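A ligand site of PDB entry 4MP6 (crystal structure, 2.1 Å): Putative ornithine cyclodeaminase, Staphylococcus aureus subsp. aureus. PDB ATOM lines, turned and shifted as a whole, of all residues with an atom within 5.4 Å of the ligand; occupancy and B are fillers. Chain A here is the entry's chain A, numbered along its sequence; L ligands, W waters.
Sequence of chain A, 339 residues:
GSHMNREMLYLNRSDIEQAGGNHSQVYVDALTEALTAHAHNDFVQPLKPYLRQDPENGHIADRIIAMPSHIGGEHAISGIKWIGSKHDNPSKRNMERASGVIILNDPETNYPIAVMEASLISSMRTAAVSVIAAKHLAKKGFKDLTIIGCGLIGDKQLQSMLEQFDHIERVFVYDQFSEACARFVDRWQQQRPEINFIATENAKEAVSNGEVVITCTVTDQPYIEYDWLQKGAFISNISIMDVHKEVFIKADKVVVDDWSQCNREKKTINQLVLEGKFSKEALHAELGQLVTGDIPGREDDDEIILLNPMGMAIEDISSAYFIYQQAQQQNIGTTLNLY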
ATOM      1  N   ARG A  63     -31.611  18.585 -32.944  1.00  0.00           N
ATOM      2  CA  ARG A  63     -32.442  17.606 -33.605  1.00  0.00           C
ATOM      3  C   ARG A  63     -33.841  17.614 -32.993  1.00  0.00           C
ATOM      4  O   ARG A  63     -34.067  18.181 -31.920  1.00  0.00           O
ATOM      5  CB  ARG A  63     -31.815  16.215 -33.481  1.00  0.00           C
ATOM      6  CG  ARG A  63     -32.026  15.530 -32.143  1.00  0.00           C
ATOM      7  CD  ARG A  63     -31.064  16.007 -31.072  1.00  0.00           C
ATOM      8  NE  ARG A  63     -31.498  15.575 -29.734  1.00  0.00           N
ATOM      9  CZ  ARG A  63     -30.711  15.036 -28.803  1.00  0.00           C
ATOM     10  NH1 ARG A  63     -29.424  14.877 -29.032  1.00  0.00           N
ATOM     11  NH2 ARG A  63     -31.220  14.670 -27.628  1.00  0.00           N
ATOM     12  N   HIS A  87     -28.963  23.016 -28.855  1.00  0.00           N
ATOM     13  CA  HIS A  87     -27.861  23.156 -27.884  1.00  0.00           C
ATOM     14  C   HIS A  87     -27.747  24.555 -27.242  1.00  0.00           C
ATOM     15  O   HIS A  87     -27.501  24.656 -26.041  1.00  0.00           O
ATOM     16  CB  HIS A  87     -26.513  22.778 -28.543  1.00  0.00           C
ATOM     17  CG  HIS A  87     -25.965  23.832 -29.450  1.00  0.00           C
ATOM     18  ND1 HIS A  87     -26.639  24.279 -30.570  1.00  0.00           N
ATOM     19  CD2 HIS A  87     -24.820  24.561 -29.398  1.00  0.00           C
ATOM     20  CE1 HIS A  87     -25.937  25.220 -31.174  1.00  0.00           C
ATOM     21  NE2 HIS A  87     -24.831  25.416 -30.479  1.00  0.00           N
ATOM     22  N   PRO A  90     -30.407  27.469 -24.107  1.00  0.00           N
ATOM     23  CA  PRO A  90     -30.191  28.135 -22.808  1.00  0.00           C
ATOM     24  C   PRO A  90     -29.163  29.267 -22.901  1.00  0.00           C
ATOM     25  O   PRO A  90     -29.449  30.372 -22.466  1.00  0.00           O
ATOM     26  CB  PRO A  90     -29.739  27.001 -21.887  1.00  0.00           C
ATOM     27  CG  PRO A  90     -30.230  25.745 -22.567  1.00  0.00           C
ATOM     28  CD  PRO A  90     -30.048  26.037 -24.032  1.00  0.00           C
ATOM     29  N   ARG A  97     -33.227  23.817 -23.230  1.00  0.00           N
ATOM     30  CA  ARG A  97     -32.677  23.151 -24.425  1.00  0.00           C
ATOM     31  C   ARG A  97     -33.745  22.305 -25.163  1.00  0.00           C
ATOM     32  O   ARG A  97     -33.927  22.453 -26.370  1.00  0.00           O
ATOM     33  CB  ARG A  97     -31.459  22.266 -24.052  1.00  0.00           C
ATOM     34  CG  ARG A  97     -31.087  21.204 -25.099  1.00  0.00           C
ATOM     35  CD  ARG A  97     -30.209  20.072 -24.545  1.00  0.00           C
ATOM     36  NE  ARG A  97     -30.860  19.164 -23.580  1.00  0.00           N
ATOM     37  CZ  ARG A  97     -31.580  18.066 -23.864  1.00  0.00           C
ATOM     38  NH1 ARG A  97     -31.797  17.730 -25.139  1.00  0.00           N
ATOM     39  NH2 ARG A  97     -32.105  17.303 -22.872  1.00  0.00           N
ATOM     40  N   ALA A  98     -34.422  21.446 -24.409  1.00  0.00           N
ATOM     41  CA  ALA A  98     -35.391  20.521 -24.963  1.00  0.00           C
ATOM     42  C   ALA A  98     -36.800  21.010 -24.711  1.00  0.00           C
ATOM     43  O   ALA A  98     -37.079  21.768 -23.751  1.00  0.00           O
ATOM     44  CB  ALA A  98     -35.198  19.125 -24.363  1.00  0.00           C
ATOM     45  N   SER A 122     -40.268  13.815 -19.617  1.00  0.00           N
ATOM     46  CA  SER A 122     -39.077  13.195 -20.156  1.00  0.00           C
ATOM     47  C   SER A 122     -37.921  13.201 -19.122  1.00  0.00           C
ATOM     48  O   SER A 122     -37.251  12.167 -18.896  1.00  0.00           O
ATOM     49  CB  SER A 122     -38.666  13.949 -21.441  1.00  0.00           C
ATOM     50  OG  SER A 122     -37.608  13.267 -22.108  1.00  0.00           O
ATOM     51  N   ARG A 125     -39.092  10.836 -16.166  1.00  0.00           N
ATOM     52  CA  ARG A 125     -38.924   9.402 -16.460  1.00  0.00           C
ATOM     53  C   ARG A 125     -37.428   9.014 -16.562  1.00  0.00           C
ATOM     54  O   ARG A 125     -37.040   7.923 -16.135  1.00  0.00           O
ATOM     55  CB  ARG A 125     -39.763   8.923 -17.672  1.00  0.00           C
ATOM     56  CG  ARG A 125     -39.367   9.431 -19.048  1.00  0.00           C
ATOM     57  CD  ARG A 125     -38.073   8.816 -19.553  1.00  0.00           C
ATOM     58  NE  ARG A 125     -38.060   8.780 -21.020  1.00  0.00           N
ATOM     59  CZ  ARG A 125     -36.975   8.741 -21.783  1.00  0.00           C
ATOM     60  NH1 ARG A 125     -35.768   8.809 -21.242  1.00  0.00           N
ATOM     61  NH2 ARG A 125     -37.102   8.655 -23.124  1.00  0.00           N
ATOM     62  N   THR A 126     -36.602   9.918 -17.058  1.00  0.00           N
ATOM     63  CA  THR A 126     -35.167   9.645 -17.175  1.00  0.00           C
ATOM     64  C   THR A 126     -34.505   9.522 -15.788  1.00  0.00           C
ATOM     65  O   THR A 126     -33.653   8.665 -15.580  1.00  0.00           O
ATOM     66  CB  THR A 126     -34.440  10.703 -18.046  1.00  0.00           C
ATOM     67  OG1 THR A 126     -35.063  10.760 -19.342  1.00  0.00           O
ATOM     68  CG2 THR A 126     -33.006  10.309 -18.252  1.00  0.00           C
ATOM     69  N   ILE A 148     -22.954  14.987 -12.623  1.00  0.00           N
ATOM     70  CA  ILE A 148     -22.120  15.780 -13.571  1.00  0.00           C
ATOM     71  C   ILE A 148     -23.011  16.456 -14.581  1.00  0.00           C
ATOM     72  O   ILE A 148     -23.726  15.775 -15.290  1.00  0.00           O
ATOM     73  CB  ILE A 148     -21.138  14.902 -14.362  1.00  0.00           C
ATOM     74  CG1 ILE A 148     -20.357  13.980 -13.421  1.00  0.00           C
ATOM     75  CG2 ILE A 148     -20.217  15.782 -15.222  1.00  0.00           C
ATOM     76  CD1 ILE A 148     -19.484  14.706 -12.405  1.00  0.00           C
ATOM     77  N   GLY A 149     -22.950  17.778 -14.652  1.00  0.00           N
ATOM     78  CA  GLY A 149     -23.851  18.537 -15.501  1.00  0.00           C
ATOM     79  C   GLY A 149     -25.075  18.998 -14.728  1.00  0.00           C
ATOM     80  O   GLY A 149     -25.831  18.190 -14.187  1.00  0.00           O
ATOM     81  N   CYS A 150     -25.276  20.304 -14.661  1.00  0.00           N
ATOM     82  CA  CYS A 150     -26.265  20.883 -13.771  1.00  0.00           C
ATOM     83  C   CYS A 150     -27.438  21.487 -14.522  1.00  0.00           C
ATOM     84  O   CYS A 150     -28.023  22.469 -14.045  1.00  0.00           O
ATOM     85  CB  CYS A 150     -25.601  21.948 -12.894  1.00  0.00           C
ATOM     86  SG  CYS A 150     -24.224  21.312 -11.918  1.00  0.00           S
ATOM     87  N   GLY A 151     -27.785  20.941 -15.685  1.00  0.00           N
ATOM     88  CA  GLY A 151     -28.936  21.441 -16.416  1.00  0.00           C
ATOM     89  C   GLY A 151     -30.209  20.840 -15.872  1.00  0.00           C
ATOM     90  O   GLY A 151     -30.245  20.359 -14.737  1.00  0.00           O
ATOM     91  N   LEU A 152     -31.265  20.872 -16.679  1.00  0.00           N
ATOM     92  CA  LEU A 152     -32.557  20.376 -16.251  1.00  0.00           C
ATOM     93  C   LEU A 152     -32.546  18.861 -15.970  1.00  0.00           C
ATOM     94  O   LEU A 152     -33.225  18.390 -15.063  1.00  0.00           O
ATOM     95  CB  LEU A 152     -33.661  20.751 -17.258  1.00  0.00           C
ATOM     96  CG  LEU A 152     -35.010  20.013 -17.091  1.00  0.00           C
ATOM     97  CD1 LEU A 152     -35.675  20.259 -15.730  1.00  0.00           C
ATOM     98  CD2 LEU A 152     -35.938  20.437 -18.199  1.00  0.00           C
ATOM     99  N   ILE A 153     -31.783  18.105 -16.759  1.00  0.00           N
ATOM    100  CA  ILE A 153     -31.691  16.680 -16.535  1.00  0.00           C
ATOM    101  C   ILE A 153     -31.025  16.408 -15.170  1.00  0.00           C
ATOM    102  O   ILE A 153     -31.570  15.645 -14.358  1.00  0.00           O
ATOM    103  CB  ILE A 153     -30.996  15.972 -17.713  1.00  0.00           C
ATOM    104  CG1 ILE A 153     -31.879  16.057 -18.983  1.00  0.00           C
ATOM    105  CG2 ILE A 153     -30.643  14.527 -17.379  1.00  0.00           C
ATOM    106  CD1 ILE A 153     -33.187  15.272 -18.915  1.00  0.00           C
ATOM    107  N   GLY A 154     -29.879  17.068 -14.919  1.00  0.00           N
ATOM    108  CA  GLY A 154     -29.179  16.975 -13.635  1.00  0.00           C
ATOM    109  C   GLY A 154     -30.067  17.284 -12.426  1.00  0.00           C
ATOM    110  O   GLY A 154     -30.135  16.491 -11.458  1.00  0.00           O
ATOM    111  N   TYR A 174     -20.350  18.564 -10.305  1.00  0.00           N
ATOM    112  CA  TYR A 174     -19.436  19.239 -11.224  1.00  0.00           C
ATOM    113  C   TYR A 174     -20.157  19.700 -12.485  1.00  0.00           C
ATOM    114  O   TYR A 174     -21.071  19.035 -12.993  1.00  0.00           O
ATOM    115  CB  TYR A 174     -18.209  18.371 -11.589  1.00  0.00           C
ATOM    116  CG  TYR A 174     -17.279  19.079 -12.564  1.00  0.00           C
ATOM    117  CD1 TYR A 174     -16.513  20.177 -12.160  1.00  0.00           C
ATOM    118  CD2 TYR A 174     -17.180  18.667 -13.893  1.00  0.00           C
ATOM    119  CE1 TYR A 174     -15.684  20.850 -13.054  1.00  0.00           C
ATOM    120  CE2 TYR A 174     -16.351  19.329 -14.804  1.00  0.00           C
ATOM    121  CZ  TYR A 174     -15.603  20.420 -14.384  1.00  0.00           C
ATOM    122  OH  TYR A 174     -14.787  21.083 -15.284  1.00  0.00           O
ATOM    123  N   ASP A 175     -19.764  20.865 -12.964  1.00  0.00           N
ATOM    124  CA  ASP A 175     -20.167  21.321 -14.266  1.00  0.00           C
ATOM    125  C   ASP A 175     -18.984  22.024 -14.913  1.00  0.00           C
ATOM    126  O   ASP A 175     -18.234  22.742 -14.239  1.00  0.00           O
ATOM    127  CB  ASP A 175     -21.377  22.244 -14.187  1.00  0.00           C
ATOM    128  CG  ASP A 175     -22.114  22.354 -15.519  1.00  0.00           C
ATOM    129  OD1 ASP A 175     -21.519  22.905 -16.455  1.00  0.00           O
ATOM    130  OD2 ASP A 175     -23.263  21.846 -15.618  1.00  0.00           O
ATOM    131  N   GLN A 176     -18.815  21.806 -16.225  1.00  0.00           N
ATOM    132  CA  GLN A 176     -17.765  22.436 -17.017  1.00  0.00           C
ATOM    133  C   GLN A 176     -17.825  23.964 -16.914  1.00  0.00           C
ATOM    134  O   GLN A 176     -16.819  24.644 -17.035  1.00  0.00           O
ATOM    135  CB  GLN A 176     -17.946  22.039 -18.479  1.00  0.00           C
ATOM    136  CG  GLN A 176     -16.696  22.141 -19.331  1.00  0.00           C
ATOM    137  CD  GLN A 176     -16.911  21.453 -20.663  1.00  0.00           C
ATOM    138  OE1 GLN A 176     -17.821  21.811 -21.430  1.00  0.00           O
ATOM    139  NE2 GLN A 176     -16.099  20.442 -20.952  1.00  0.00           N
ATOM    140  N   PHE A 177     -19.038  24.456 -16.734  1.00  0.00           N
ATOM    141  CA  PHE A 177     -19.304  25.855 -16.537  1.00  0.00           C
ATOM    142  C   PHE A 177     -19.440  26.088 -15.031  1.00  0.00           C
ATOM    143  O   PHE A 177     -20.470  25.760 -14.424  1.00  0.00           O
ATOM    144  CB  PHE A 177     -20.585  26.222 -17.301  1.00  0.00           C
ATOM    145  CG  PHE A 177     -20.931  27.683 -17.300  1.00  0.00           C
ATOM    146  CD1 PHE A 177     -19.924  28.661 -17.365  1.00  0.00           C
ATOM    147  CD2 PHE A 177     -22.263  28.088 -17.256  1.00  0.00           C
ATOM    148  CE1 PHE A 177     -20.258  30.011 -17.363  1.00  0.00           C
ATOM    149  CE2 PHE A 177     -22.601  29.425 -17.257  1.00  0.00           C
ATOM    150  CZ  PHE A 177     -21.589  30.386 -17.323  1.00  0.00           C
ATOM    151  N   ALA A 180     -22.646  27.684 -13.431  1.00  0.00           N
ATOM    152  CA  ALA A 180     -23.790  26.774 -13.459  1.00  0.00           C
ATOM    153  C   ALA A 180     -23.781  25.877 -12.220  1.00  0.00           C
ATOM    154  O   ALA A 180     -24.773  25.783 -11.502  1.00  0.00           O
ATOM    155  CB  ALA A 180     -23.759  25.938 -14.729  1.00  0.00           C
ATOM    156  N   CYS A 216     -24.948  13.911 -16.763  1.00  0.00           N
ATOM    157  CA  CYS A 216     -26.052  14.704 -17.243  1.00  0.00           C
ATOM    158  C   CYS A 216     -25.533  15.874 -18.117  1.00  0.00           C
ATOM    159  O   CYS A 216     -26.060  17.003 -18.033  1.00  0.00           O
ATOM    160  CB  CYS A 216     -26.883  15.213 -16.044  1.00  0.00           C
ATOM    161  SG  CYS A 216     -27.315  13.974 -14.754  1.00  0.00           S
ATOM    162  N   THR A 217     -24.517  15.589 -18.935  1.00  0.00           N
ATOM    163  CA  THR A 217     -23.905  16.611 -19.796  1.00  0.00           C
ATOM    164  C   THR A 217     -24.379  16.567 -21.263  1.00  0.00           C
ATOM    165  O   THR A 217     -25.271  15.803 -21.623  1.00  0.00           O
ATOM    166  CB  THR A 217     -22.362  16.520 -19.804  1.00  0.00           C
ATOM    167  OG1 THR A 217     -21.955  15.404 -20.601  1.00  0.00           O
ATOM    168  CG2 THR A 217     -21.781  16.390 -18.413  1.00  0.00           C
ATOM    169  N   VAL A 218     -23.770  17.423 -22.100  1.00  0.00           N
ATOM    170  CA  VAL A 218     -23.957  17.368 -23.545  1.00  0.00           C
ATOM    171  C   VAL A 218     -22.628  17.123 -24.278  1.00  0.00           C
ATOM    172  O   VAL A 218     -22.426  17.608 -25.366  1.00  0.00           O
ATOM    173  CB  VAL A 218     -24.590  18.680 -24.058  1.00  0.00           C
ATOM    174  CG1 VAL A 218     -26.034  18.799 -23.578  1.00  0.00           C
ATOM    175  CG2 VAL A 218     -23.732  19.870 -23.618  1.00  0.00           C
ATOM    176  N   THR A 219     -21.712  16.379 -23.678  1.00  0.00           N
ATOM    177  CA  THR A 219     -20.426  16.099 -24.340  1.00  0.00           C
ATOM    178  C   THR A 219     -20.613  15.144 -25.535  1.00  0.00           C
ATOM    179  O   THR A 219     -21.612  14.432 -25.619  1.00  0.00           O
ATOM    180  CB  THR A 219     -19.378  15.537 -23.344  1.00  0.00           C
ATOM    181  OG1 THR A 219     -18.127  15.391 -24.012  1.00  0.00           O
ATOM    182  CG2 THR A 219     -19.777  14.188 -22.770  1.00  0.00           C
ATOM    183  N   TYR A 223     -14.870  11.533 -20.968  1.00  0.00           N
ATOM    184  CA  TYR A 223     -13.866  12.080 -20.037  1.00  0.00           C
ATOM    185  C   TYR A 223     -13.741  11.206 -18.788  1.00  0.00           C
ATOM    186  O   TYR A 223     -12.785  11.340 -18.030  1.00  0.00           O
ATOM    187  CB  TYR A 223     -14.181  13.542 -19.643  1.00  0.00           C
ATOM    188  CG  TYR A 223     -15.557  13.661 -19.043  1.00  0.00           C
ATOM    189  CD1 TYR A 223     -15.792  13.313 -17.710  1.00  0.00           C
ATOM    190  CD2 TYR A 223     -16.638  14.047 -19.830  1.00  0.00           C
ATOM    191  CE1 TYR A 223     -17.069  13.382 -17.184  1.00  0.00           C
ATOM    192  CE2 TYR A 223     -17.905  14.113 -19.302  1.00  0.00           C
ATOM    193  CZ  TYR A 223     -18.115  13.792 -17.986  1.00  0.00           C
ATOM    194  OH  TYR A 223     -19.382  13.847 -17.474  1.00  0.00           O
ATOM    195  N   ASN A 237     -25.262   6.245 -16.853  1.00  0.00           N
ATOM    196  CA  ASN A 237     -24.668   7.087 -17.907  1.00  0.00           C
ATOM    197  C   ASN A 237     -25.770   7.708 -18.775  1.00  0.00           C
ATOM    198  O   ASN A 237     -25.843   7.491 -20.007  1.00  0.00           O
ATOM    199  CB  ASN A 237     -23.701   6.243 -18.720  1.00  0.00           C
ATOM    200  CG  ASN A 237     -22.931   7.035 -19.763  1.00  0.00           C
ATOM    201  OD1 ASN A 237     -22.626   8.220 -19.576  1.00  0.00           O
ATOM    202  ND2 ASN A 237     -22.590   6.372 -20.868  1.00  0.00           N
ATOM    203  N   ILE A 238     -26.620   8.476 -18.103  1.00  0.00           N
ATOM    204  CA  ILE A 238     -27.743   9.117 -18.734  1.00  0.00           C
ATOM    205  C   ILE A 238     -27.347   9.948 -19.974  1.00  0.00           C
ATOM    206  O   ILE A 238     -28.082   9.962 -20.944  1.00  0.00           O
ATOM    207  CB  ILE A 238     -28.542   9.943 -17.705  1.00  0.00           C
ATOM    208  CG1 ILE A 238     -29.142   9.029 -16.604  1.00  0.00           C
ATOM    209  CG2 ILE A 238     -29.621  10.757 -18.376  1.00  0.00           C
ATOM    210  CD1 ILE A 238     -30.221   8.071 -17.078  1.00  0.00           C
ATOM    211  N   SER A 239     -26.206  10.647 -19.951  1.00  0.00           N
ATOM    212  CA  SER A 239     -25.904  11.487 -21.114  1.00  0.00           C
ATOM    213  C   SER A 239     -24.945  10.824 -22.140  1.00  0.00           C
ATOM    214  O   SER A 239     -24.415  11.475 -23.059  1.00  0.00           O
ATOM    215  CB  SER A 239     -25.410  12.846 -20.680  1.00  0.00           C
ATOM    216  OG  SER A 239     -24.249  12.728 -19.935  1.00  0.00           O
ATOM    217  N   ILE A 240     -24.718   9.518 -21.921  1.00  0.00           N
ATOM    218  CA  ILE A 240     -24.258   8.535 -22.935  1.00  0.00           C
ATOM    219  C   ILE A 240     -22.804   8.679 -23.324  1.00  0.00           C
ATOM    220  O   ILE A 240     -22.017   7.758 -23.170  1.00  0.00           O
ATOM    221  CB  ILE A 240     -25.217   8.450 -24.166  1.00  0.00           C
ATOM    222  CG1 ILE A 240     -26.596   7.921 -23.741  1.00  0.00           C
ATOM    223  CG2 ILE A 240     -24.659   7.564 -25.290  1.00  0.00           C
ATOM    224  CD1 ILE A 240     -26.618   6.517 -23.175  1.00  0.00           C
ATOM    225  N   PRO A 309     -28.220   3.743 -20.732  1.00  0.00           N
ATOM    226  CA  PRO A 309     -29.619   3.696 -21.182  1.00  0.00           C
ATOM    227  C   PRO A 309     -29.903   4.707 -22.295  1.00  0.00           C
ATOM    228  O   PRO A 309     -29.831   5.902 -22.045  1.00  0.00           O
ATOM    229  CB  PRO A 309     -30.404   4.037 -19.897  1.00  0.00           C
ATOM    230  CG  PRO A 309     -29.463   4.938 -19.101  1.00  0.00           C
ATOM    231  CD  PRO A 309     -28.043   4.719 -19.635  1.00  0.00           C
ATOM    232  N   MET A 310     -30.236   4.234 -23.494  1.00  0.00           N
ATOM    233  CA  MET A 310     -30.450   5.112 -24.651  1.00  0.00           C
ATOM    234  C   MET A 310     -31.707   5.972 -24.568  1.00  0.00           C
ATOM    235  O   MET A 310     -31.791   7.007 -25.229  1.00  0.00           O
ATOM    236  CB  MET A 310     -30.499   4.284 -25.938  1.00  0.00           C
ATOM    237  CG  MET A 310     -29.141   4.016 -26.561  1.00  0.00           C
ATOM    238  SD  MET A 310     -28.372   5.503 -27.257  1.00  0.00           S
ATOM    239  CE  MET A 310     -29.536   5.965 -28.548  1.00  0.00           C
ATOM    240  N   GLY A 311     -32.687   5.532 -23.767  1.00  0.00           N
ATOM    241  CA  GLY A 311     -34.013   6.173 -23.697  1.00  0.00           C
ATOM    242  C   GLY A 311     -35.008   5.387 -24.544  1.00  0.00           C
ATOM    243  O   GLY A 311     -34.695   5.027 -25.690  1.00  0.00           O
ATOM    244  N   MET A 312     -36.178   5.080 -23.963  1.00  0.00           N
ATOM    245  CA  MET A 312     -37.193   4.251 -24.628  1.00  0.00           C
ATOM    246  C   MET A 312     -38.561   4.949 -24.607  1.00  0.00           C
ATOM    247  O   MET A 312     -39.005   5.435 -23.580  1.00  0.00           O
ATOM    248  CB  MET A 312     -37.326   2.879 -23.964  1.00  0.00           C
ATOM    249  CG  MET A 312     -36.078   2.014 -24.021  1.00  0.00           C
ATOM    250  SD  MET A 312     -36.476   0.337 -23.507  1.00  0.00           S
ATOM    251  CE  MET A 312     -36.925   0.502 -21.783  1.00  0.00           C
ATOM    252  N   GLU A 315     -41.213   4.339 -21.853  1.00  0.00           N
ATOM    253  CA  GLU A 315     -41.037   5.119 -20.616  1.00  0.00           C
ATOM    254  C   GLU A 315     -41.844   6.432 -20.667  1.00  0.00           C
ATOM    255  O   GLU A 315     -42.525   6.772 -19.702  1.00  0.00           O
ATOM    256  CB  GLU A 315     -39.562   5.395 -20.375  1.00  0.00           C
ATOM    257  CG  GLU A 315     -38.742   4.133 -20.214  1.00  0.00           C
ATOM    258  CD  GLU A 315     -37.261   4.360 -20.370  1.00  0.00           C
ATOM    259  OE1 GLU A 315     -36.862   5.450 -20.859  1.00  0.00           O
ATOM    260  OE2 GLU A 315     -36.494   3.426 -20.029  1.00  0.00           O
HETATM  261  P1  LIG L   1     -28.593  21.312 -20.492  1.00  0.00           P
HETATM  262  O1  LIG L   1     -28.072  22.163 -21.635  1.00  0.00           O
HETATM  263  O2  LIG L   1     -29.767  21.797 -19.662  1.00  0.00           O
HETATM  264  O3  LIG L   1     -27.344  21.053 -19.487  1.00  0.00           O
HETATM  265  C1  LIG L   1     -26.143  20.329 -19.791  1.00  0.00           C
HETATM  266  C2  LIG L   1     -25.124  20.732 -18.706  1.00  0.00           C
HETATM  267  O4  LIG L   1     -23.903  19.993 -18.774  1.00  0.00           O
HETATM  268  C3  LIG L   1     -24.720  22.203 -18.823  1.00  0.00           C
HETATM  269  O5  LIG L   1     -24.739  22.799 -17.529  1.00  0.00           O
HETATM  270  C4  LIG L   1     -23.324  22.179 -19.402  1.00  0.00           C
HETATM  271  O6  LIG L   1     -22.589  23.362 -19.054  1.00  0.00           O
HETATM  272  C5  LIG L   1     -22.772  20.891 -18.797  1.00  0.00           C
HETATM  273  N1  LIG L   1     -21.672  20.234 -19.551  1.00  0.00           N
HETATM  274  C6  LIG L   1     -21.556  20.112 -20.902  1.00  0.00           C
HETATM  275  N2  LIG L   1     -20.458  19.390 -21.232  1.00  0.00           N
HETATM  276  C7  LIG L   1     -19.837  19.058 -20.079  1.00  0.00           C
HETATM  277  C8  LIG L   1     -18.606  18.322 -19.707  1.00  0.00           C
HETATM  278  N3  LIG L   1     -17.821  17.801 -20.661  1.00  0.00           N
HETATM  279  N4  LIG L   1     -18.311  18.176 -18.381  1.00  0.00           N
HETATM  280  C9  LIG L   1     -19.091  18.686 -17.421  1.00  0.00           C
HETATM  281  N5  LIG L   1     -20.230  19.372 -17.711  1.00  0.00           N
HETATM  282  C10 LIG L   1     -20.630  19.597 -18.983  1.00  0.00           C
HETATM  283  O7  LIG L   1     -28.941  19.827 -21.080  1.00  0.00           O
HETATM  284  P2  LIG L   1     -30.008  18.863 -20.334  1.00  0.00           P
HETATM  285  O8  LIG L   1     -31.414  19.155 -20.812  1.00  0.00           O
HETATM  286  O9  LIG L   1     -29.942  18.957 -18.831  1.00  0.00           O
HETATM  287  O10 LIG L   1     -29.629  17.434 -20.928  1.00  0.00           O
HETATM  288  C11 LIG L   1     -28.479  16.728 -20.456  1.00  0.00           C
HETATM  289  C12 LIG L   1     -28.321  15.440 -21.264  1.00  0.00           C
HETATM  290  O11 LIG L   1     -29.316  14.469 -20.893  1.00  0.00           O
HETATM  291  C13 LIG L   1     -28.372  15.576 -22.784  1.00  0.00           C
HETATM  292  O12 LIG L   1     -27.154  14.987 -23.211  1.00  0.00           O
HETATM  293  C14 LIG L   1     -29.492  14.646 -23.229  1.00  0.00           C
HETATM  294  O13 LIG L   1     -29.204  14.034 -24.522  1.00  0.00           O
HETATM  295  C15 LIG L   1     -29.507  13.638 -22.061  1.00  0.00           C
HETATM  296  N6  LIG L   1     -30.761  12.865 -21.929  1.00  0.00           N
HETATM  297  C16 LIG L   1     -30.674  11.521 -21.949  1.00  0.00           C
HETATM  298  C17 LIG L   1     -31.826  10.754 -21.821  1.00  0.00           C
HETATM  299  C18 LIG L   1     -31.729   9.245 -21.865  1.00  0.00           C
HETATM  300  O14 LIG L   1     -30.632   8.663 -21.856  1.00  0.00           O
HETATM  301  N7  LIG L   1     -32.877   8.581 -21.982  1.00  0.00           N
HETATM  302  C19 LIG L   1     -33.079  11.371 -21.686  1.00  0.00           C
HETATM  303  C20 LIG L   1     -33.131  12.755 -21.656  1.00  0.00           C
HETATM  304  C21 LIG L   1     -31.942  13.483 -21.771  1.00  0.00           C
HETATM  305  O   HOH W   1     -21.223  22.329 -23.520  1.00  0.00           O
HETATM  306  O   HOH W   2     -28.056  18.307 -16.994  1.00  0.00           O
HETATM  307  O   HOH W   3     -29.462  24.426 -18.410  1.00  0.00           O
HETATM  308  O   HOH W   4     -27.789  11.925 -24.377  1.00  0.00           O
HETATM  309  O   HOH W   5     -18.657  18.331 -23.924  1.00  0.00           O
HETATM  310  O   HOH W   6     -27.581  15.548 -26.097  1.00  0.00           O
HETATM  311  O   HOH W   7     -33.693  20.831 -21.532  1.00  0.00           O
HETATM  312  O   HOH W   8     -32.054  22.823 -20.461  1.00  0.00           O
HETATM  313  O   HOH W   9     -26.283  24.716 -17.289  1.00  0.00           O
HETATM  314  O   HOH W  10     -33.466   6.664 -20.193  1.00  0.00           O
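Water W8 bridges an oxygen (O2) of the ligand (2.6 Å) and the backbone NH (N) of Arg 97 (3.2 Å). Water W10 lies within hydrogen-bond range of N7 of the ligand (2.7 Å) and NH1 of Arg 125 (3.3 Å). Water W2 lies within hydrogen-bond range of the backbone carbonyl oxygen (O) of Cys 216 (2.6 Å), an oxygen (O9) of the ligand (2.7 Å), the backbone NH (N) of Gly 151 (3.0 Å) and the backbone NH (N) of Gly 154 (3.0 Å). Water W7 lies within hydrogen-bond range of an oxygen (O8) of the ligand (2.9 Å), the backbone NH of Ala 98 (3.0 Å) and the backbone NH of Arg 97 (3.5 Å). Water W5 lies within hydrogen-bond range of the side-chain hydroxyl of Thr 219 (3.0 Å) and a nitrogen (N2) of the ligand (3.4 Å).
The side-chain hydroxyl (OG) of Ser 239 sits at hydrogen-bond distance from the backbone NH (N) of Thr 217, at 3.0 Å. The side-chain hydroxyl (OG1) of Thr 217 lies within hydrogen-bond range of the backbone NH (N) of Thr 219 (3.2 Å). The backbone NH of Cys 150 lies within hydrogen-bond range of the side-chain carboxylate of Asp 175 (2.7 Å). OD1 of Asp 175 sits at hydrogen-bond distance from N of Phe 177 (2.9 Å). The side-chain hydroxyl of Thr 126 sits at hydrogen-bond distance from the guanidinium group of Arg 125 (2.8 Å). OG1 of Thr 126 sits at hydrogen-bond distance from O of Ser 122 (2.6 Å). N of Cys 216 lies within hydrogen-bond range of OG of Ser 239 (3.5 Å). The backbone carbonyl oxygen (O) of Tyr 174 lies within hydrogen-bond range of the backbone NH (N) of Gly 149, at 2.8 Å.
O of Thr 217 lies within hydrogen-bond range of O12 of the ligand, at 2.6 Å. The side-chain carboxylate (OD2) of Asp 175 lies within hydrogen-bond range of an oxygen (O5) of the ligand, at 2.6 Å. An oxygen (O8) of the ligand is in salt-bridge range of the guanidinium group of Arg 97, at 2.8 Å. N of Ile 153 is in hydrogen-bond range of O9 of the ligand (2.9 Å). A nitrogen (N5) of the ligand is in hydrogen-bond range of the backbone NH (N) of Gln 176 (3.2 Å). The side-chain amide nitrogen (NE2) of Gln 176 lies close to a nitrogen (N3) of the ligand, at 3.2 Å. The backbone NH of Leu 152 is in hydrogen-bond range of an oxygen (O9) of the ligand (3.2 Å).
N7 of the ligand sits close to NH1 of Arg 125 (3.0 Å). An oxygen (O14) of the ligand sits close to the backbone carbonyl oxygen (O) of Ile 238 (3.0 Å). The backbone carbonyl oxygen of Pro 309 lies close to an oxygen (O14) of the ligand, 2.9 Å away. Residues that only touch the ligand: Arg 63 (3.8 Å), Thr 126 (3.1 Å), Ile 148 (3.8 Å), Gly 149 (3.6 Å), Cys 150 (3.8 Å), Gly 151 (3.4 Å), Tyr 174 (3.8 Å), Phe 177 (3.9 Å), Cys 216 (3.4 Å), Val 218 (3.5 Å), Thr 219 (3.8 Å), Tyr 223 (3.9 Å), Ser 239 (3.7 Å), Met 310 (3.8 Å) and Gly 311 (3.2 Å). Hydrophobic or aromatic side chains that line the ligand: Ile 148, Ile 153, Tyr 174, Phe 177, Val 218, Tyr 223 and Ile 238.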
